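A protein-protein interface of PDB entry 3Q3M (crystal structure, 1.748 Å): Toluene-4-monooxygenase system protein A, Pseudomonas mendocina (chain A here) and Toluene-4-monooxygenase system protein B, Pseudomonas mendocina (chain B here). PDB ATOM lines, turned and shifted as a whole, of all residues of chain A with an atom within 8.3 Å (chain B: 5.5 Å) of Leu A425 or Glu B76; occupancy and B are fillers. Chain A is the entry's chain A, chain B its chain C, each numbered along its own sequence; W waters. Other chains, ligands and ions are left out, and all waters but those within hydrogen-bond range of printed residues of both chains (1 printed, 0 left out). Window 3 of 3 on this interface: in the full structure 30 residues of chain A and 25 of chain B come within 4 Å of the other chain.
ND1 of His B7 sits at hydrogen-bond distance from OG of Ser A395 (2.8 Å).
NE2 of His A427 sits at hydrogen-bond distance from O of Thr B75 (2.8 Å).
O of Pro B5 is in hydrogen-bond range of N of Thr B75.
The backbone NH (N) of Asn A398 sits at hydrogen-bond distance from the backbone carbonyl oxygen (O) of His A427, at 2.9 Å.
The side-chain carboxylate of Glu B76 sits at hydrogen-bond distance from the side-chain amide nitrogen of Asn B73, at 2.7 Å.
O of His B7 sits at hydrogen-bond distance from N of Ile B78 (2.8 Å).
O of Glu B76 lies within hydrogen-bond range of N of His B7.
The side-chain hydroxyl (OG) of Ser A418 lies within hydrogen-bond range of a ring nitrogen (ND1) of His A427, 2.8 Å away.
Leu A425 touches Thr B75 (CD2 to O, 3.6 Å).
Glu B76 touches Leu A425 (CG to CD2, 3.8 Å).
NE2 of His A427 touches CD2 of His B7, 3.7 Å away.
His A427 touches Val B77 (CE1 to CG2, 3.7 Å).
Pro B5 touches Leu A455 (CB to CD2, 3.96 Å).
Leu A455 touches Thr B75 (CD1 to CG2, 3.8 Å).
Val A416 touches none of the printed residues of chain B.
Of the printed residues of chain B, Leu A425 touches Thr B75 and Glu B76.
Phe A428 touches none of the printed residues of chain B.
Printed residues of chain B within 4 Å of Leu A455: Pro B5 (3.96 Å) and Thr B75 (3.8 Å).
Of the printed residues of chain A, Pro B5 touches Leu A455.
Printed residues of chain A within 4 Å of His B7: Ser A395 and His A427.
Of the printed residues of chain A, Thr B75 touches Leu A425, His A427 and Leu A455.
Of chain A, only Leu A425 comes within 4 Å of Glu B76.
Printed residues of chain A within 4 Å of Val B77: His A427.
The nearest residue of chain B that does not touch Leu A425 is Pro B74 (4.6 Å).
Hydrophobic or aromatic side chains of chain B within 4 Å of the printed part of chain A: Pro B5, His B7 and Val B77.
Of the 20 printed residues of chain A, 4 touch a printed residue of chain B.
Along chain A the printed residues that touch a printed residue of chain B span positions 395 to 455.
Among the printed residues, no Asp or Glu carboxylate lies within 4 Å of a Lys or Arg side-chain nitrogen of the other chain.
Water W1 bridges O of Leu A425 (2.6 Å) and OG1 of Thr B75 (2.7 Å).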
ATOM      1  N   SER A 395     -23.449  -5.678 -10.096  1.00  0.00           N
ATOM      2  CA  SER A 395     -23.853  -6.992 -10.597  1.00  0.00           C
ATOM      3  C   SER A 395     -24.083  -7.914  -9.394  1.00  0.00           C
ATOM      4  O   SER A 395     -23.339  -7.830  -8.415  1.00  0.00           O
ATOM      5  CB  SER A 395     -22.749  -7.573 -11.493  1.00  0.00           C
ATOM      6  OG  SER A 395     -22.364  -6.629 -12.482  1.00  0.00           O
ATOM      7  N   VAL A 396     -25.097  -8.784  -9.464  1.00  0.00           N
ATOM      8  CA  VAL A 396     -25.533  -9.543  -8.282  1.00  0.00           C
ATOM      9  C   VAL A 396     -25.486 -11.052  -8.519  1.00  0.00           C
ATOM     10  O   VAL A 396     -25.828 -11.514  -9.589  1.00  0.00           O
ATOM     11  CB  VAL A 396     -26.973  -9.135  -7.857  1.00  0.00           C
ATOM     12  CG1 VAL A 396     -27.535 -10.057  -6.750  1.00  0.00           C
ATOM     13  CG2 VAL A 396     -26.990  -7.680  -7.395  1.00  0.00           C
ATOM     14  N   ASN A 398     -26.693 -14.826  -8.616  1.00  0.00           N
ATOM     15  CA  ASN A 398     -27.985 -15.499  -8.800  1.00  0.00           C
ATOM     16  C   ASN A 398     -28.291 -16.537  -7.718  1.00  0.00           C
ATOM     17  O   ASN A 398     -29.387 -17.096  -7.685  1.00  0.00           O
ATOM     18  CB  ASN A 398     -28.082 -16.153 -10.193  1.00  0.00           C
ATOM     19  CG  ASN A 398     -28.533 -15.174 -11.258  1.00  0.00           C
ATOM     20  OD1 ASN A 398     -27.753 -14.793 -12.127  1.00  0.00           O
ATOM     21  ND2 ASN A 398     -29.792 -14.736 -11.178  1.00  0.00           N
ATOM     22  N   VAL A 416     -16.186 -14.157 -11.686  1.00  0.00           N
ATOM     23  CA  VAL A 416     -17.602 -14.511 -11.750  1.00  0.00           C
ATOM     24  C   VAL A 416     -17.694 -15.896 -12.388  1.00  0.00           C
ATOM     25  O   VAL A 416     -17.010 -16.195 -13.375  1.00  0.00           O
ATOM     26  CB  VAL A 416     -18.368 -13.488 -12.623  1.00  0.00           C
ATOM     27  CG1 VAL A 416     -19.845 -13.836 -12.743  1.00  0.00           C
ATOM     28  CG2 VAL A 416     -18.176 -12.089 -12.065  1.00  0.00           C
ATOM     29  N   PHE A 417     -18.518 -16.760 -11.807  1.00  0.00           N
ATOM     30  CA  PHE A 417     -18.688 -18.119 -12.319  1.00  0.00           C
ATOM     31  C   PHE A 417     -20.063 -18.201 -12.956  1.00  0.00           C
ATOM     32  O   PHE A 417     -21.069 -18.177 -12.263  1.00  0.00           O
ATOM     33  CB  PHE A 417     -18.527 -19.115 -11.163  1.00  0.00           C
ATOM     34  CG  PHE A 417     -17.197 -19.009 -10.506  1.00  0.00           C
ATOM     35  CD1 PHE A 417     -16.137 -19.784 -10.929  1.00  0.00           C
ATOM     36  CD2 PHE A 417     -16.985 -18.077  -9.502  1.00  0.00           C
ATOM     37  CE1 PHE A 417     -14.878 -19.662 -10.323  1.00  0.00           C
ATOM     38  CE2 PHE A 417     -15.740 -17.938  -8.901  1.00  0.00           C
ATOM     39  CZ  PHE A 417     -14.685 -18.732  -9.310  1.00  0.00           C
ATOM     40  N   SER A 418     -20.100 -18.280 -14.284  1.00  0.00           N
ATOM     41  CA  SER A 418     -21.377 -18.165 -14.985  1.00  0.00           C
ATOM     42  C   SER A 418     -21.868 -19.494 -15.519  1.00  0.00           C
ATOM     43  O   SER A 418     -21.134 -20.498 -15.538  1.00  0.00           O
ATOM     44  CB  SER A 418     -21.266 -17.148 -16.108  1.00  0.00           C
ATOM     45  OG  SER A 418     -20.763 -15.918 -15.603  1.00  0.00           O
ATOM     46  N   LEU A 419     -23.123 -19.498 -15.952  1.00  0.00           N
ATOM     47  CA  LEU A 419     -23.771 -20.723 -16.415  1.00  0.00           C
ATOM     48  C   LEU A 419     -24.932 -20.392 -17.341  1.00  0.00           C
ATOM     49  O   LEU A 419     -25.786 -19.551 -17.001  1.00  0.00           O
ATOM     50  CB  LEU A 419     -24.306 -21.521 -15.214  1.00  0.00           C
ATOM     51  CG  LEU A 419     -25.034 -22.826 -15.560  1.00  0.00           C
ATOM     52  CD1 LEU A 419     -24.065 -23.870 -16.098  1.00  0.00           C
ATOM     53  CD2 LEU A 419     -25.755 -23.358 -14.322  1.00  0.00           C
ATOM     54  N   GLU A 420     -24.947 -21.018 -18.525  1.00  0.00           N
ATOM     55  CA  GLU A 420     -26.125 -20.982 -19.384  1.00  0.00           C
ATOM     56  C   GLU A 420     -26.987 -22.165 -19.040  1.00  0.00           C
ATOM     57  O   GLU A 420     -26.505 -23.289 -18.974  1.00  0.00           O
ATOM     58  CB  GLU A 420     -25.747 -21.092 -20.871  1.00  0.00           C
ATOM     59  CG  GLU A 420     -24.992 -19.903 -21.401  1.00  0.00           C
ATOM     60  CD  GLU A 420     -24.616 -20.103 -22.863  1.00  0.00           C
ATOM     61  OE1 GLU A 420     -25.547 -20.085 -23.695  1.00  0.00           O
ATOM     62  OE2 GLU A 420     -23.415 -20.330 -23.152  1.00  0.00           O
ATOM     63  N   HIS A 421     -28.279 -21.931 -18.860  1.00  0.00           N
ATOM     64  CA  HIS A 421     -29.180 -23.010 -18.455  1.00  0.00           C
ATOM     65  C   HIS A 421     -30.588 -22.634 -18.890  1.00  0.00           C
ATOM     66  O   HIS A 421     -31.070 -21.545 -18.548  1.00  0.00           O
ATOM     67  CB  HIS A 421     -29.118 -23.168 -16.934  1.00  0.00           C
ATOM     68  CG  HIS A 421     -30.197 -24.031 -16.346  1.00  0.00           C
ATOM     69  ND1 HIS A 421     -30.176 -25.409 -16.414  1.00  0.00           N
ATOM     70  CD2 HIS A 421     -31.314 -23.709 -15.642  1.00  0.00           C
ATOM     71  CE1 HIS A 421     -31.236 -25.897 -15.791  1.00  0.00           C
ATOM     72  NE2 HIS A 421     -31.944 -24.884 -15.316  1.00  0.00           N
ATOM     73  N   ASN A 422     -31.235 -23.513 -19.657  1.00  0.00           N
ATOM     74  CA  ASN A 422     -32.605 -23.261 -20.123  1.00  0.00           C
ATOM     75  C   ASN A 422     -32.830 -21.843 -20.643  1.00  0.00           C
ATOM     76  O   ASN A 422     -33.791 -21.171 -20.252  1.00  0.00           O
ATOM     77  CB  ASN A 422     -33.608 -23.528 -18.989  1.00  0.00           C
ATOM     78  CG  ASN A 422     -33.725 -25.003 -18.648  1.00  0.00           C
ATOM     79  OD1 ASN A 422     -33.170 -25.862 -19.345  1.00  0.00           O
ATOM     80  ND2 ASN A 422     -34.457 -25.309 -17.577  1.00  0.00           N
ATOM     81  N   GLY A 423     -31.926 -21.375 -21.492  1.00  0.00           N
ATOM     82  CA  GLY A 423     -32.124 -20.118 -22.190  1.00  0.00           C
ATOM     83  C   GLY A 423     -31.857 -18.861 -21.391  1.00  0.00           C
ATOM     84  O   GLY A 423     -32.223 -17.758 -21.823  1.00  0.00           O
ATOM     85  N   ARG A 424     -31.244 -19.013 -20.221  1.00  0.00           N
ATOM     86  CA  ARG A 424     -30.845 -17.859 -19.429  1.00  0.00           C
ATOM     87  C   ARG A 424     -29.366 -17.927 -19.084  1.00  0.00           C
ATOM     88  O   ARG A 424     -28.833 -19.008 -18.925  1.00  0.00           O
ATOM     89  CB  ARG A 424     -31.630 -17.799 -18.116  1.00  0.00           C
ATOM     90  CG  ARG A 424     -32.925 -17.014 -18.176  1.00  0.00           C
ATOM     91  CD  ARG A 424     -33.593 -16.954 -16.785  1.00  0.00           C
ATOM     92  NE  ARG A 424     -32.852 -16.184 -15.774  1.00  0.00           N
ATOM     93  CZ  ARG A 424     -33.167 -16.189 -14.476  1.00  0.00           C
ATOM     94  NH1 ARG A 424     -34.186 -16.933 -14.062  1.00  0.00           N
ATOM     95  NH2 ARG A 424     -32.481 -15.465 -13.595  1.00  0.00           N
ATOM     96  N   LEU A 425     -28.732 -16.758 -18.953  1.00  0.00           N
ATOM     97  CA  LEU A 425     -27.362 -16.636 -18.467  1.00  0.00           C
ATOM     98  C   LEU A 425     -27.384 -16.220 -16.981  1.00  0.00           C
ATOM     99  O   LEU A 425     -27.881 -15.129 -16.629  1.00  0.00           O
ATOM    100  CB  LEU A 425     -26.570 -15.611 -19.290  1.00  0.00           C
ATOM    101  CG  LEU A 425     -25.113 -15.452 -18.830  1.00  0.00           C
ATOM    102  CD1 LEU A 425     -24.326 -16.771 -18.941  1.00  0.00           C
ATOM    103  CD2 LEU A 425     -24.399 -14.335 -19.641  1.00  0.00           C
ATOM    104  N   TYR A 426     -26.857 -17.099 -16.120  1.00  0.00           N
ATOM    105  CA  TYR A 426     -26.773 -16.845 -14.687  1.00  0.00           C
ATOM    106  C   TYR A 426     -25.314 -16.547 -14.303  1.00  0.00           C
ATOM    107  O   TYR A 426     -24.379 -17.050 -14.928  1.00  0.00           O
ATOM    108  CB  TYR A 426     -27.212 -18.083 -13.901  1.00  0.00           C
ATOM    109  CG  TYR A 426     -28.612 -18.609 -14.214  1.00  0.00           C
ATOM    110  CD1 TYR A 426     -29.668 -18.372 -13.352  1.00  0.00           C
ATOM    111  CD2 TYR A 426     -28.850 -19.385 -15.351  1.00  0.00           C
ATOM    112  CE1 TYR A 426     -30.948 -18.884 -13.623  1.00  0.00           C
ATOM    113  CE2 TYR A 426     -30.108 -19.876 -15.634  1.00  0.00           C
ATOM    114  CZ  TYR A 426     -31.153 -19.628 -14.767  1.00  0.00           C
ATOM    115  OH  TYR A 426     -32.386 -20.157 -15.066  1.00  0.00           O
ATOM    116  N   HIS A 427     -25.135 -15.770 -13.243  1.00  0.00           N
ATOM    117  CA  HIS A 427     -23.800 -15.419 -12.774  1.00  0.00           C
ATOM    118  C   HIS A 427     -23.730 -15.691 -11.273  1.00  0.00           C
ATOM    119  O   HIS A 427     -24.619 -15.278 -10.528  1.00  0.00           O
ATOM    120  CB  HIS A 427     -23.511 -13.930 -13.023  1.00  0.00           C
ATOM    121  CG  HIS A 427     -23.638 -13.516 -14.457  1.00  0.00           C
ATOM    122  ND1 HIS A 427     -22.817 -14.011 -15.448  1.00  0.00           N
ATOM    123  CD2 HIS A 427     -24.506 -12.673 -15.070  1.00  0.00           C
ATOM    124  CE1 HIS A 427     -23.163 -13.480 -16.608  1.00  0.00           C
ATOM    125  NE2 HIS A 427     -24.190 -12.668 -16.408  1.00  0.00           N
ATOM    126  N   PHE A 428     -22.670 -16.367 -10.827  1.00  0.00           N
ATOM    127  CA  PHE A 428     -22.522 -16.689  -9.420  1.00  0.00           C
ATOM    128  C   PHE A 428     -21.221 -16.111  -8.873  1.00  0.00           C
ATOM    129  O   PHE A 428     -20.230 -15.978  -9.628  1.00  0.00           O
ATOM    130  CB  PHE A 428     -22.572 -18.222  -9.247  1.00  0.00           C
ATOM    131  CG  PHE A 428     -23.852 -18.823  -9.758  1.00  0.00           C
ATOM    132  CD1 PHE A 428     -25.014 -18.748  -9.001  1.00  0.00           C
ATOM    133  CD2 PHE A 428     -23.909 -19.442 -11.012  1.00  0.00           C
ATOM    134  CE1 PHE A 428     -26.209 -19.276  -9.467  1.00  0.00           C
ATOM    135  CE2 PHE A 428     -25.113 -19.979 -11.486  1.00  0.00           C
ATOM    136  CZ  PHE A 428     -26.266 -19.896 -10.710  1.00  0.00           C
ATOM    137  N   PHE A 437     -26.497 -24.235  -7.038  1.00  0.00           N
ATOM    138  CA  PHE A 437     -27.536 -24.147  -8.065  1.00  0.00           C
ATOM    139  C   PHE A 437     -27.658 -25.491  -8.784  1.00  0.00           C
ATOM    140  O   PHE A 437     -28.760 -26.015  -8.983  1.00  0.00           O
ATOM    141  CB  PHE A 437     -27.177 -23.026  -9.063  1.00  0.00           C
ATOM    142  CG  PHE A 437     -28.186 -22.804 -10.161  1.00  0.00           C
ATOM    143  CD1 PHE A 437     -29.142 -21.803 -10.048  1.00  0.00           C
ATOM    144  CD2 PHE A 437     -28.142 -23.553 -11.335  1.00  0.00           C
ATOM    145  CE1 PHE A 437     -30.058 -21.574 -11.078  1.00  0.00           C
ATOM    146  CE2 PHE A 437     -29.066 -23.321 -12.370  1.00  0.00           C
ATOM    147  CZ  PHE A 437     -29.995 -22.324 -12.247  1.00  0.00           C
ATOM    148  N   ASN A 449     -33.068 -12.363  -9.816  1.00  0.00           N
ATOM    149  CA  ASN A 449     -32.473 -11.499  -8.799  1.00  0.00           C
ATOM    150  C   ASN A 449     -32.820 -10.050  -9.115  1.00  0.00           C
ATOM    151  O   ASN A 449     -33.416  -9.767 -10.139  1.00  0.00           O
ATOM    152  CB  ASN A 449     -30.957 -11.754  -8.557  1.00  0.00           C
ATOM    153  CG  ASN A 449     -30.051 -11.246  -9.662  1.00  0.00           C
ATOM    154  OD1 ASN A 449     -30.406 -10.369 -10.440  1.00  0.00           O
ATOM    155  ND2 ASN A 449     -28.831 -11.803  -9.717  1.00  0.00           N
ATOM    156  N   ASP A 452     -31.722  -8.896 -12.460  1.00  0.00           N
ATOM    157  CA  ASP A 452     -32.520  -9.531 -13.510  1.00  0.00           C
ATOM    158  C   ASP A 452     -33.854  -8.812 -13.660  1.00  0.00           C
ATOM    159  O   ASP A 452     -34.323  -8.593 -14.767  1.00  0.00           O
ATOM    160  CB  ASP A 452     -32.806 -10.998 -13.162  1.00  0.00           C
ATOM    161  CG  ASP A 452     -31.550 -11.845 -13.087  1.00  0.00           C
ATOM    162  OD1 ASP A 452     -30.607 -11.629 -13.882  1.00  0.00           O
ATOM    163  OD2 ASP A 452     -31.508 -12.745 -12.215  1.00  0.00           O
ATOM    164  N   LEU A 455     -33.444  -5.440 -15.378  1.00  0.00           N
ATOM    165  CA  LEU A 455     -33.235  -5.578 -16.823  1.00  0.00           C
ATOM    166  C   LEU A 455     -34.489  -6.035 -17.580  1.00  0.00           C
ATOM    167  O   LEU A 455     -34.657  -5.725 -18.775  1.00  0.00           O
ATOM    168  CB  LEU A 455     -32.047  -6.502 -17.125  1.00  0.00           C
ATOM    169  CG  LEU A 455     -30.683  -5.939 -16.707  1.00  0.00           C
ATOM    170  CD1 LEU A 455     -29.568  -6.969 -16.928  1.00  0.00           C
ATOM    171  CD2 LEU A 455     -30.399  -4.683 -17.485  1.00  0.00           C
ATOM    172  N   PRO B   5     -26.835  -4.177 -22.310  1.00  0.00           N
ATOM    173  CA  PRO B   5     -26.320  -4.313 -20.946  1.00  0.00           C
ATOM    174  C   PRO B   5     -25.114  -5.264 -20.889  1.00  0.00           C
ATOM    175  O   PRO B   5     -25.112  -6.314 -21.538  1.00  0.00           O
ATOM    176  CB  PRO B   5     -27.515  -4.904 -20.188  1.00  0.00           C
ATOM    177  CG  PRO B   5     -28.228  -5.705 -21.204  1.00  0.00           C
ATOM    178  CD  PRO B   5     -28.098  -4.915 -22.497  1.00  0.00           C
ATOM    179  N   VAL B   6     -24.078  -4.855 -20.171  1.00  0.00           N
ATOM    180  CA  VAL B   6     -22.990  -5.764 -19.828  1.00  0.00           C
ATOM    181  C   VAL B   6     -22.715  -5.730 -18.337  1.00  0.00           C
ATOM    182  O   VAL B   6     -23.132  -4.816 -17.632  1.00  0.00           O
ATOM    183  CB  VAL B   6     -21.663  -5.442 -20.582  1.00  0.00           C
ATOM    184  CG1 VAL B   6     -21.824  -5.670 -22.071  1.00  0.00           C
ATOM    185  CG2 VAL B   6     -21.182  -4.034 -20.288  1.00  0.00           C
ATOM    186  N   HIS B   7     -22.002  -6.733 -17.852  1.00  0.00           N
ATOM    187  CA  HIS B   7     -21.505  -6.671 -16.492  1.00  0.00           C
ATOM    188  C   HIS B   7     -20.009  -6.465 -16.607  1.00  0.00           C
ATOM    189  O   HIS B   7     -19.331  -7.206 -17.316  1.00  0.00           O
ATOM    190  CB  HIS B   7     -21.847  -7.957 -15.740  1.00  0.00           C
ATOM    191  CG  HIS B   7     -23.312  -8.118 -15.484  1.00  0.00           C
ATOM    192  ND1 HIS B   7     -24.000  -7.325 -14.590  1.00  0.00           N
ATOM    193  CD2 HIS B   7     -24.226  -8.951 -16.032  1.00  0.00           C
ATOM    194  CE1 HIS B   7     -25.278  -7.672 -14.589  1.00  0.00           C
ATOM    195  NE2 HIS B   7     -25.444  -8.647 -15.467  1.00  0.00           N
ATOM    196  N   LYS B  54     -13.310 -10.317 -22.855  1.00  0.00           N
ATOM    197  CA  LYS B  54     -14.254 -11.173 -22.146  1.00  0.00           C
ATOM    198  C   LYS B  54     -13.673 -11.545 -20.784  1.00  0.00           C
ATOM    199  O   LYS B  54     -12.465 -11.738 -20.658  1.00  0.00           O
ATOM    200  CB  LYS B  54     -14.562 -12.444 -22.937  1.00  0.00           C
ATOM    201  CG  LYS B  54     -15.336 -12.193 -24.210  1.00  0.00           C
ATOM    202  CD  LYS B  54     -15.928 -13.476 -24.778  1.00  0.00           C
ATOM    203  CE  LYS B  54     -17.129 -13.943 -23.948  1.00  0.00           C
ATOM    204  NZ  LYS B  54     -17.747 -15.212 -24.480  1.00  0.00           N
ATOM    205  N   GLY B  71     -19.326 -10.126 -31.047  1.00  0.00           N
ATOM    206  CA  GLY B  71     -19.931 -11.404 -30.720  1.00  0.00           C
ATOM    207  C   GLY B  71     -20.442 -11.479 -29.280  1.00  0.00           C
ATOM    208  O   GLY B  71     -21.102 -12.444 -28.911  1.00  0.00           O
ATOM    209  N   LEU B  72     -20.145 -10.470 -28.462  1.00  0.00           N
ATOM    210  CA  LEU B  72     -20.641 -10.467 -27.076  1.00  0.00           C
ATOM    211  C   LEU B  72     -22.166 -10.592 -27.041  1.00  0.00           C
ATOM    212  O   LEU B  72     -22.858 -10.058 -27.915  1.00  0.00           O
ATOM    213  CB  LEU B  72     -20.224  -9.186 -26.344  1.00  0.00           C
ATOM    214  CG  LEU B  72     -18.774  -9.090 -25.872  1.00  0.00           C
ATOM    215  CD1 LEU B  72     -18.432  -7.657 -25.448  1.00  0.00           C
ATOM    216  CD2 LEU B  72     -18.533 -10.065 -24.710  1.00  0.00           C
ATOM    217  N   ASN B  73     -22.692 -11.284 -26.039  1.00  0.00           N
ATOM    218  CA  ASN B  73     -24.136 -11.343 -25.844  1.00  0.00           C
ATOM    219  C   ASN B  73     -24.527 -10.467 -24.681  1.00  0.00           C
ATOM    220  O   ASN B  73     -23.717 -10.251 -23.770  1.00  0.00           O
ATOM    221  CB  ASN B  73     -24.592 -12.771 -25.571  1.00  0.00           C
ATOM    222  CG  ASN B  73     -24.338 -13.686 -26.744  1.00  0.00           C
ATOM    223  OD1 ASN B  73     -24.751 -13.396 -27.861  1.00  0.00           O
ATOM    224  ND2 ASN B  73     -23.641 -14.793 -26.500  1.00  0.00           N
ATOM    225  N   PRO B  74     -25.772  -9.965 -24.688  1.00  0.00           N
ATOM    226  CA  PRO B  74     -26.213  -9.106 -23.581  1.00  0.00           C
ATOM    227  C   PRO B  74     -26.048  -9.809 -22.239  1.00  0.00           C
ATOM    228  O   PRO B  74     -26.358 -10.998 -22.111  1.00  0.00           O
ATOM    229  CB  PRO B  74     -27.694  -8.878 -23.889  1.00  0.00           C
ATOM    230  CG  PRO B  74     -27.767  -8.963 -25.363  1.00  0.00           C
ATOM    231  CD  PRO B  74     -26.788 -10.050 -25.748  1.00  0.00           C
ATOM    232  N   THR B  75     -25.585  -9.044 -21.259  1.00  0.00           N
ATOM    233  CA  THR B  75     -25.378  -9.476 -19.871  1.00  0.00           C
ATOM    234  C   THR B  75     -24.174 -10.403 -19.686  1.00  0.00           C
ATOM    235  O   THR B  75     -23.977 -10.945 -18.595  1.00  0.00           O
ATOM    236  CB  THR B  75     -26.662 -10.073 -19.169  1.00  0.00           C
ATOM    237  OG1 THR B  75     -26.884 -11.437 -19.577  1.00  0.00           O
ATOM    238  CG2 THR B  75     -27.906  -9.231 -19.473  1.00  0.00           C
ATOM    239  N   GLU B  76     -23.360 -10.586 -20.729  1.00  0.00           N
ATOM    240  CA  GLU B  76     -22.078 -11.277 -20.534  1.00  0.00           C
ATOM    241  C   GLU B  76     -21.120 -10.405 -19.711  1.00  0.00           C
ATOM    242  O   GLU B  76     -21.290  -9.178 -19.645  1.00  0.00           O
ATOM    243  CB  GLU B  76     -21.464 -11.726 -21.880  1.00  0.00           C
ATOM    244  CG  GLU B  76     -22.181 -13.001 -22.407  1.00  0.00           C
ATOM    245  CD  GLU B  76     -21.709 -13.515 -23.776  1.00  0.00           C
ATOM    246  OE1 GLU B  76     -20.898 -12.856 -24.448  1.00  0.00           O
ATOM    247  OE2 GLU B  76     -22.188 -14.596 -24.193  1.00  0.00           O
ATOM    248  N   VAL B  77     -20.124 -11.026 -19.077  1.00  0.00           N
ATOM    249  CA  VAL B  77     -19.180 -10.276 -18.246  1.00  0.00           C
ATOM    250  C   VAL B  77     -17.923  -9.903 -19.048  1.00  0.00           C
ATOM    251  O   VAL B  77     -17.376 -10.731 -19.760  1.00  0.00           O
ATOM    252  CB  VAL B  77     -18.750 -11.107 -17.014  1.00  0.00           C
ATOM    253  CG1 VAL B  77     -17.895 -10.258 -16.063  1.00  0.00           C
ATOM    254  CG2 VAL B  77     -19.973 -11.709 -16.314  1.00  0.00           C
ATOM    255  N   ILE B  78     -17.500  -8.646 -18.947  1.00  0.00           N
ATOM    256  CA  ILE B  78     -16.233  -8.196 -19.515  1.00  0.00           C
ATOM    257  C   ILE B  78     -15.333  -7.621 -18.437  1.00  0.00           C
ATOM    258  O   ILE B  78     -15.816  -7.206 -17.395  1.00  0.00           O
ATOM    259  CB  ILE B  78     -16.449  -7.096 -20.588  1.00  0.00           C
ATOM    260  CG1 ILE B  78     -17.158  -5.871 -19.977  1.00  0.00           C
ATOM    261  CG2 ILE B  78     -17.250  -7.656 -21.736  1.00  0.00           C
ATOM    262  CD1 ILE B  78     -17.340  -4.693 -20.975  1.00  0.00           C
HETATM  263  O   HOH W   1     -27.959 -12.634 -17.389  1.00  0.00           O
